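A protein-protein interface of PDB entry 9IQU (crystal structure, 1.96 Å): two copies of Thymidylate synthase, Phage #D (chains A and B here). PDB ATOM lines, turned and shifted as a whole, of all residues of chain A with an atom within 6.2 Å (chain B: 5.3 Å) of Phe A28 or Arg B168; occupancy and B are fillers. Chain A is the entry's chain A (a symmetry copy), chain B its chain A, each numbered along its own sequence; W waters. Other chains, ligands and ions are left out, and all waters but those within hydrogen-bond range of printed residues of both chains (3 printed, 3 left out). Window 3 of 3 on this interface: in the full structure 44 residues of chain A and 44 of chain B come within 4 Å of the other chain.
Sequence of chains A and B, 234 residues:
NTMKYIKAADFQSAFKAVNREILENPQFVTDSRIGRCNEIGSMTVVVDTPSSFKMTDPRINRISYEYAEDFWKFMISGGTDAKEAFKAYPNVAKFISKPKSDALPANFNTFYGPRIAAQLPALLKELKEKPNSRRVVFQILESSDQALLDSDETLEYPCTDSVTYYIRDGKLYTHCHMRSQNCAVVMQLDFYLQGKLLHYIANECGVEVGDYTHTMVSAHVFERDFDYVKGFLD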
ATOM      1  N   LYS A   4      15.405 -10.993  27.870  1.00  0.00           N
ATOM      2  CA  LYS A   4      15.269 -11.941  26.774  1.00  0.00           C
ATOM      3  C   LYS A   4      14.765 -11.290  25.501  1.00  0.00           C
ATOM      4  O   LYS A   4      14.711 -11.931  24.447  1.00  0.00           O
ATOM      5  CB  LYS A   4      14.336 -13.071  27.173  1.00  0.00           C
ATOM      6  CG  LYS A   4      14.903 -14.008  28.224  1.00  0.00           C
ATOM      7  CD  LYS A   4      14.079 -15.283  28.264  1.00  0.00           C
ATOM      8  CE  LYS A   4      14.715 -16.356  29.122  1.00  0.00           C
ATOM      9  NZ  LYS A   4      14.209 -17.672  28.675  1.00  0.00           N
ATOM     10  N   PRO A  26      23.366 -14.894  32.282  1.00  0.00           N
ATOM     11  CA  PRO A  26      22.918 -16.091  31.551  1.00  0.00           C
ATOM     12  C   PRO A  26      21.734 -16.779  32.233  1.00  0.00           C
ATOM     13  O   PRO A  26      21.606 -16.675  33.450  1.00  0.00           O
ATOM     14  CB  PRO A  26      24.150 -17.005  31.579  1.00  0.00           C
ATOM     15  CG  PRO A  26      24.887 -16.582  32.804  1.00  0.00           C
ATOM     16  CD  PRO A  26      24.686 -15.094  32.906  1.00  0.00           C
ATOM     17  N   GLN A  27      20.890 -17.467  31.469  1.00  0.00           N
ATOM     18  CA  GLN A  27      19.854 -18.300  32.078  1.00  0.00           C
ATOM     19  C   GLN A  27      20.487 -19.629  32.542  1.00  0.00           C
ATOM     20  O   GLN A  27      20.200 -20.142  33.623  1.00  0.00           O
ATOM     21  CB  GLN A  27      18.704 -18.548  31.087  1.00  0.00           C
ATOM     22  CG  GLN A  27      17.543 -19.395  31.660  1.00  0.00           C
ATOM     23  CD  GLN A  27      16.369 -19.488  30.704  1.00  0.00           C
ATOM     24  OE1 GLN A  27      16.448 -19.016  29.565  1.00  0.00           O
ATOM     25  NE2 GLN A  27      15.274 -20.103  31.153  1.00  0.00           N
ATOM     26  N   PHE A  28      21.380 -20.172  31.725  1.00  0.00           N
ATOM     27  CA  PHE A  28      22.032 -21.436  32.041  1.00  0.00           C
ATOM     28  C   PHE A  28      23.538 -21.288  31.834  1.00  0.00           C
ATOM     29  O   PHE A  28      23.989 -20.563  30.945  1.00  0.00           O
ATOM     30  CB  PHE A  28      21.534 -22.581  31.150  1.00  0.00           C
ATOM     31  CG  PHE A  28      20.040 -22.664  30.982  1.00  0.00           C
ATOM     32  CD1 PHE A  28      19.244 -23.256  31.953  1.00  0.00           C
ATOM     33  CD2 PHE A  28      19.438 -22.215  29.808  1.00  0.00           C
ATOM     34  CE1 PHE A  28      17.846 -23.364  31.779  1.00  0.00           C
ATOM     35  CE2 PHE A  28      18.044 -22.327  29.624  1.00  0.00           C
ATOM     36  CZ  PHE A  28      17.251 -22.907  30.614  1.00  0.00           C
ATOM     37  N   VAL A  29      24.308 -21.983  32.654  1.00  0.00           N
ATOM     38  CA  VAL A  29      25.716 -22.242  32.377  1.00  0.00           C
ATOM     39  C   VAL A  29      25.851 -23.748  32.212  1.00  0.00           C
ATOM     40  O   VAL A  29      25.687 -24.507  33.173  1.00  0.00           O
ATOM     41  CB  VAL A  29      26.638 -21.689  33.475  1.00  0.00           C
ATOM     42  CG1 VAL A  29      28.072 -21.743  33.021  1.00  0.00           C
ATOM     43  CG2 VAL A  29      26.287 -20.249  33.773  1.00  0.00           C
ATOM     44  N   THR A  30      26.138 -24.184  30.993  1.00  0.00           N
ATOM     45  CA  THR A  30      25.926 -25.577  30.632  1.00  0.00           C
ATOM     46  C   THR A  30      26.989 -26.206  29.714  1.00  0.00           C
ATOM     47  O   THR A  30      27.590 -25.541  28.859  1.00  0.00           O
ATOM     48  CB  THR A  30      24.542 -25.721  29.969  1.00  0.00           C
ATOM     49  OG1 THR A  30      24.276 -27.100  29.665  1.00  0.00           O
ATOM     50  CG2 THR A  30      24.446 -24.859  28.706  1.00  0.00           C
ATOM     51  N   CYS A  37      29.270 -23.333  27.839  1.00  0.00           N
ATOM     52  CA  CYS A  37      28.791 -22.038  27.381  1.00  0.00           C
ATOM     53  C   CYS A  37      27.805 -21.414  28.363  1.00  0.00           C
ATOM     54  O   CYS A  37      27.212 -22.110  29.206  1.00  0.00           O
ATOM     55  CB  CYS A  37      28.146 -22.164  25.990  1.00  0.00           C
ATOM     56  SG  CYS A  37      26.699 -23.262  25.917  1.00  0.00           S
ATOM     57  N   ASN A  38      27.693 -20.090  28.277  1.00  0.00           N
ATOM     58  CA  ASN A  38      26.602 -19.340  28.880  1.00  0.00           C
ATOM     59  C   ASN A  38      25.470 -19.334  27.869  1.00  0.00           C
ATOM     60  O   ASN A  38      25.730 -19.250  26.660  1.00  0.00           O
ATOM     61  CB  ASN A  38      27.021 -17.913  29.229  1.00  0.00           C
ATOM     62  CG  ASN A  38      27.820 -17.830  30.535  1.00  0.00           C
ATOM     63  OD1 ASN A  38      28.410 -18.812  30.992  1.00  0.00           O
ATOM     64  ND2 ASN A  38      27.805 -16.661  31.150  1.00  0.00           N
ATOM     65  N   GLU A  39      24.226 -19.421  28.340  1.00  0.00           N
ATOM     66  CA  GLU A  39      23.100 -19.608  27.422  1.00  0.00           C
ATOM     67  C   GLU A  39      21.856 -18.888  27.949  1.00  0.00           C
ATOM     68  O   GLU A  39      21.623 -18.816  29.155  1.00  0.00           O
ATOM     69  CB  GLU A  39      22.834 -21.116  27.213  1.00  0.00           C
ATOM     70  CG  GLU A  39      21.626 -21.519  26.314  1.00  0.00           C
ATOM     71  CD  GLU A  39      21.465 -23.055  26.201  1.00  0.00           C
ATOM     72  OE1 GLU A  39      21.219 -23.698  27.242  1.00  0.00           O
ATOM     73  OE2 GLU A  39      21.562 -23.626  25.089  1.00  0.00           O
ATOM     74  N   ILE A  40      21.068 -18.347  27.029  1.00  0.00           N
ATOM     75  CA  ILE A  40      19.777 -17.766  27.347  1.00  0.00           C
ATOM     76  C   ILE A  40      18.806 -18.423  26.378  1.00  0.00           C
ATOM     77  O   ILE A  40      19.033 -18.408  25.170  1.00  0.00           O
ATOM     78  CB  ILE A  40      19.774 -16.222  27.235  1.00  0.00           C
ATOM     79  CG1 ILE A  40      20.734 -15.584  28.250  1.00  0.00           C
ATOM     80  CG2 ILE A  40      18.364 -15.661  27.449  1.00  0.00           C
ATOM     81  CD1 ILE A  40      20.899 -14.085  28.072  1.00  0.00           C
ATOM     82  N   GLY A  41      17.749 -19.036  26.908  1.00  0.00           N
ATOM     83  CA  GLY A  41      16.756 -19.661  26.066  1.00  0.00           C
ATOM     84  C   GLY A  41      15.726 -18.696  25.535  1.00  0.00           C
ATOM     85  O   GLY A  41      15.310 -17.755  26.232  1.00  0.00           O
ATOM     86  N   SER A 218      18.188 -21.345  21.490  1.00  0.00           N
ATOM     87  CA  SER A 218      19.416 -21.330  22.283  1.00  0.00           C
ATOM     88  C   SER A 218      20.295 -20.200  21.812  1.00  0.00           C
ATOM     89  O   SER A 218      20.784 -20.233  20.690  1.00  0.00           O
ATOM     90  CB  SER A 218      20.191 -22.636  22.172  1.00  0.00           C
ATOM     91  OG  SER A 218      21.494 -22.478  22.740  1.00  0.00           O
ATOM     92  N   ASN B 132      22.167 -32.033  27.192  1.00  0.00           N
ATOM     93  CA  ASN B 132      22.106 -30.588  26.957  1.00  0.00           C
ATOM     94  C   ASN B 132      22.060 -30.277  25.463  1.00  0.00           C
ATOM     95  O   ASN B 132      22.546 -29.232  25.016  1.00  0.00           O
ATOM     96  CB  ASN B 132      23.300 -29.876  27.605  1.00  0.00           C
ATOM     97  CG  ASN B 132      23.386 -30.121  29.113  1.00  0.00           C
ATOM     98  OD1 ASN B 132      22.387 -30.063  29.808  1.00  0.00           O
ATOM     99  ND2 ASN B 132      24.585 -30.393  29.610  1.00  0.00           N
ATOM    100  N   SER B 133      21.466 -31.191  24.699  1.00  0.00           N
ATOM    101  CA  SER B 133      21.321 -31.019  23.253  1.00  0.00           C
ATOM    102  C   SER B 133      20.546 -29.755  22.897  1.00  0.00           C
ATOM    103  O   SER B 133      19.618 -29.347  23.610  1.00  0.00           O
ATOM    104  CB  SER B 133      20.623 -32.233  22.635  1.00  0.00           C
ATOM    105  OG  SER B 133      20.318 -32.015  21.267  1.00  0.00           O
ATOM    106  N   ARG B 134      20.944 -29.150  21.788  1.00  0.00           N
ATOM    107  CA  ARG B 134      20.225 -28.022  21.199  1.00  0.00           C
ATOM    108  C   ARG B 134      19.449 -28.465  19.957  1.00  0.00           C
ATOM    109  O   ARG B 134      18.859 -27.631  19.270  1.00  0.00           O
ATOM    110  CB  ARG B 134      21.202 -26.903  20.827  1.00  0.00           C
ATOM    111  CG  ARG B 134      21.750 -26.098  21.992  1.00  0.00           C
ATOM    112  CD  ARG B 134      22.955 -25.224  21.563  1.00  0.00           C
ATOM    113  NE  ARG B 134      24.057 -26.005  20.999  1.00  0.00           N
ATOM    114  CZ  ARG B 134      25.300 -25.984  21.471  1.00  0.00           C
ATOM    115  NH1 ARG B 134      25.645 -25.207  22.489  1.00  0.00           N
ATOM    116  NH2 ARG B 134      26.218 -26.768  20.918  1.00  0.00           N
ATOM    117  N   TYR B 166      14.210 -28.750  24.919  1.00  0.00           N
ATOM    118  CA  TYR B 166      15.558 -28.953  25.449  1.00  0.00           C
ATOM    119  C   TYR B 166      15.483 -29.093  26.957  1.00  0.00           C
ATOM    120  O   TYR B 166      14.582 -28.535  27.616  1.00  0.00           O
ATOM    121  CB  TYR B 166      16.506 -27.805  25.028  1.00  0.00           C
ATOM    122  CG  TYR B 166      16.149 -26.439  25.586  1.00  0.00           C
ATOM    123  CD1 TYR B 166      15.295 -25.578  24.889  1.00  0.00           C
ATOM    124  CD2 TYR B 166      16.684 -25.998  26.788  1.00  0.00           C
ATOM    125  CE1 TYR B 166      14.979 -24.314  25.387  1.00  0.00           C
ATOM    126  CE2 TYR B 166      16.369 -24.744  27.301  1.00  0.00           C
ATOM    127  CZ  TYR B 166      15.525 -23.906  26.595  1.00  0.00           C
ATOM    128  OH  TYR B 166      15.212 -22.678  27.123  1.00  0.00           O
ATOM    129  N   ILE B 167      16.426 -29.863  27.495  1.00  0.00           N
ATOM    130  CA  ILE B 167      16.465 -30.168  28.917  1.00  0.00           C
ATOM    131  C   ILE B 167      17.743 -29.604  29.527  1.00  0.00           C
ATOM    132  O   ILE B 167      18.835 -29.925  29.076  1.00  0.00           O
ATOM    133  CB  ILE B 167      16.369 -31.688  29.151  1.00  0.00           C
ATOM    134  CG1 ILE B 167      14.964 -32.198  28.807  1.00  0.00           C
ATOM    135  CG2 ILE B 167      16.721 -32.029  30.609  1.00  0.00           C
ATOM    136  CD1 ILE B 167      14.919 -33.701  28.540  1.00  0.00           C
ATOM    137  N   ARG B 168      17.596 -28.743  30.529  1.00  0.00           N
ATOM    138  CA  ARG B 168      18.722 -28.256  31.304  1.00  0.00           C
ATOM    139  C   ARG B 168      18.418 -28.476  32.788  1.00  0.00           C
ATOM    140  O   ARG B 168      17.315 -28.139  33.247  1.00  0.00           O
ATOM    141  CB  ARG B 168      18.976 -26.764  31.058  1.00  0.00           C
ATOM    142  CG  ARG B 168      19.175 -26.348  29.618  1.00  0.00           C
ATOM    143  CD  ARG B 168      20.530 -26.773  29.041  1.00  0.00           C
ATOM    144  NE  ARG B 168      20.694 -26.262  27.679  1.00  0.00           N
ATOM    145  CZ  ARG B 168      20.313 -26.912  26.587  1.00  0.00           C
ATOM    146  NH1 ARG B 168      19.804 -28.136  26.648  1.00  0.00           N
ATOM    147  NH2 ARG B 168      20.412 -26.312  25.404  1.00  0.00           N
ATOM    148  N   ASP B 169      19.399 -28.991  33.534  1.00  0.00           N
ATOM    149  CA  ASP B 169      19.261 -29.188  34.985  1.00  0.00           C
ATOM    150  C   ASP B 169      17.918 -29.806  35.390  1.00  0.00           C
ATOM    151  O   ASP B 169      17.202 -29.292  36.259  1.00  0.00           O
ATOM    152  CB  ASP B 169      19.454 -27.858  35.709  1.00  0.00           C
ATOM    153  CG  ASP B 169      20.833 -27.259  35.467  1.00  0.00           C
ATOM    154  OD1 ASP B 169      21.799 -28.036  35.293  1.00  0.00           O
ATOM    155  OD2 ASP B 169      20.931 -26.012  35.396  1.00  0.00           O
ATOM    156  N   GLY B 170      17.567 -30.897  34.737  1.00  0.00           N
ATOM    157  CA  GLY B 170      16.404 -31.671  35.126  1.00  0.00           C
ATOM    158  C   GLY B 170      15.057 -31.139  34.665  1.00  0.00           C
ATOM    159  O   GLY B 170      14.025 -31.711  35.025  1.00  0.00           O
ATOM    160  N   LYS B 171      15.045 -30.052  33.889  1.00  0.00           N
ATOM    161  CA  LYS B 171      13.773 -29.430  33.464  1.00  0.00           C
ATOM    162  C   LYS B 171      13.619 -29.340  31.945  1.00  0.00           C
ATOM    163  O   LYS B 171      14.567 -29.034  31.230  1.00  0.00           O
ATOM    164  CB  LYS B 171      13.623 -28.026  34.071  1.00  0.00           C
ATOM    165  CG  LYS B 171      13.365 -28.024  35.582  1.00  0.00           C
ATOM    166  CD  LYS B 171      13.140 -26.602  36.121  1.00  0.00           C
ATOM    167  CE  LYS B 171      12.691 -26.622  37.587  1.00  0.00           C
ATOM    168  NZ  LYS B 171      13.109 -27.897  38.263  1.00  0.00           N
ATOM    169  N   TYR B 173      12.243 -27.504  28.731  1.00  0.00           N
ATOM    170  CA  TYR B 173      11.847 -26.198  28.227  1.00  0.00           C
ATOM    171  C   TYR B 173      11.348 -26.376  26.811  1.00  0.00           C
ATOM    172  O   TYR B 173      11.898 -27.188  26.067  1.00  0.00           O
ATOM    173  CB  TYR B 173      13.018 -25.203  28.261  1.00  0.00           C
ATOM    174  CG  TYR B 173      13.482 -24.904  29.664  1.00  0.00           C
ATOM    175  CD1 TYR B 173      14.427 -25.706  30.291  1.00  0.00           C
ATOM    176  CD2 TYR B 173      12.934 -23.859  30.382  1.00  0.00           C
ATOM    177  CE1 TYR B 173      14.824 -25.449  31.583  1.00  0.00           C
ATOM    178  CE2 TYR B 173      13.327 -23.602  31.678  1.00  0.00           C
ATOM    179  CZ  TYR B 173      14.273 -24.405  32.274  1.00  0.00           C
ATOM    180  OH  TYR B 173      14.685 -24.168  33.576  1.00  0.00           O
HETATM  181  O   HOH W   1      23.812 -24.460  24.617  1.00  0.00           O
HETATM  182  O   HOH W   2      15.326 -21.169  33.802  1.00  0.00           O
HETATM  183  O   HOH W   3      22.990 -23.350  34.792  1.00  0.00           O
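ND2 of Asn B132 lies close to OG1 of Thr A30 (3.3 Å). The guanidinium group (NE) of Arg B168 lies within salt-bridge range of the side-chain carboxylate (OE1) of Glu A39.
The backbone carbonyl oxygen of Asn B132 lies close to the guanidinium group of Arg B168 (3.4 Å). The guanidinium group of Arg B168 sits at hydrogen-bond distance from the backbone carbonyl oxygen of Ser B133 (3.3 Å). The backbone carbonyl oxygen (O) of Tyr B166 lies within hydrogen-bond range of the backbone NH (N) of Tyr B173. The side-chain amide oxygen (OE1) of Gln A27 is in hydrogen-bond range of the backbone NH (N) of Gly A41. N of Thr A30 is in hydrogen-bond range of O of Cys A37, at 2.9 Å. The side-chain hydroxyl of Ser A218 is in hydrogen-bond range of the side-chain carboxylate of Glu A39 (2.6 Å).
CE2 of Phe A28 touches CE2 of Tyr B166, at 3.7 Å. Arg B168 touches Phe A28. Phe A28 touches Tyr B173. OG1 of Thr A30 touches CD of Arg B168 (3.8 Å). Glu A39 touches Arg B134 (OE2 to CG, 3.97 Å). Tyr B166 touches Gly A41. Ser A218 touches Arg B134.
Of chain B, only Tyr B166, Arg B168 and Tyr B173 come within 4 Å of Phe A28. Of the printed residues of chain B, Gly A41 touches Tyr B166 (3.6 Å). Printed residues of chain A within 4 Å of Asn B132: Thr A30 (3.2 Å). Of chain A, only Phe A28 (3.6 Å), Thr A30 (3.8 Å) and Glu A39 (2.7 Å) come within 4 Å of Arg B168. Of the printed residues of chain A, Tyr B173 touches Phe A28. The nearest residue of chain B that does not touch Phe A28 is Asp B169 (4.7 Å). The nearest residue of chain A that does not touch Arg B168 is Ser A218 (4.8 Å). The nearest printed residue of chain B that does not touch Ser A218 is Arg B168 (4.8 Å).
Printed residues of chain A that touch a printed residue of chain B: Phe A28, Thr A30, Glu A39, Gly A41 and Ser A218. Hydrophobic or aromatic side chains of chain A within 4 Å of the printed part of chain B: Phe A28. Hydrophobic or aromatic side chains of chain B within 4 Å of the printed part of chain A: Tyr B166 and Tyr B173. Along chain B the printed residues that touch a printed residue of chain A span positions 132 to 173.
No position is printed for both chains. Of the 9 pairs that touch across the chains among the printed residues, none has its exchanged pair printed and touching as well.
Water W1 lies within hydrogen-bond range of the side-chain carboxylate (OE2) of Glu A39, the guanidinium group (NH1) of Arg B134 and the side-chain sulfur (SG) of Cys A37. Water W2 bridges NE2 of Gln A27 (2.9 Å) and OH of Tyr B173 (3.1 Å). Water W3 lies within hydrogen-bond range of N of Val A29 (2.9 Å) and OD2 of Asp B169 (3.4 Å).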
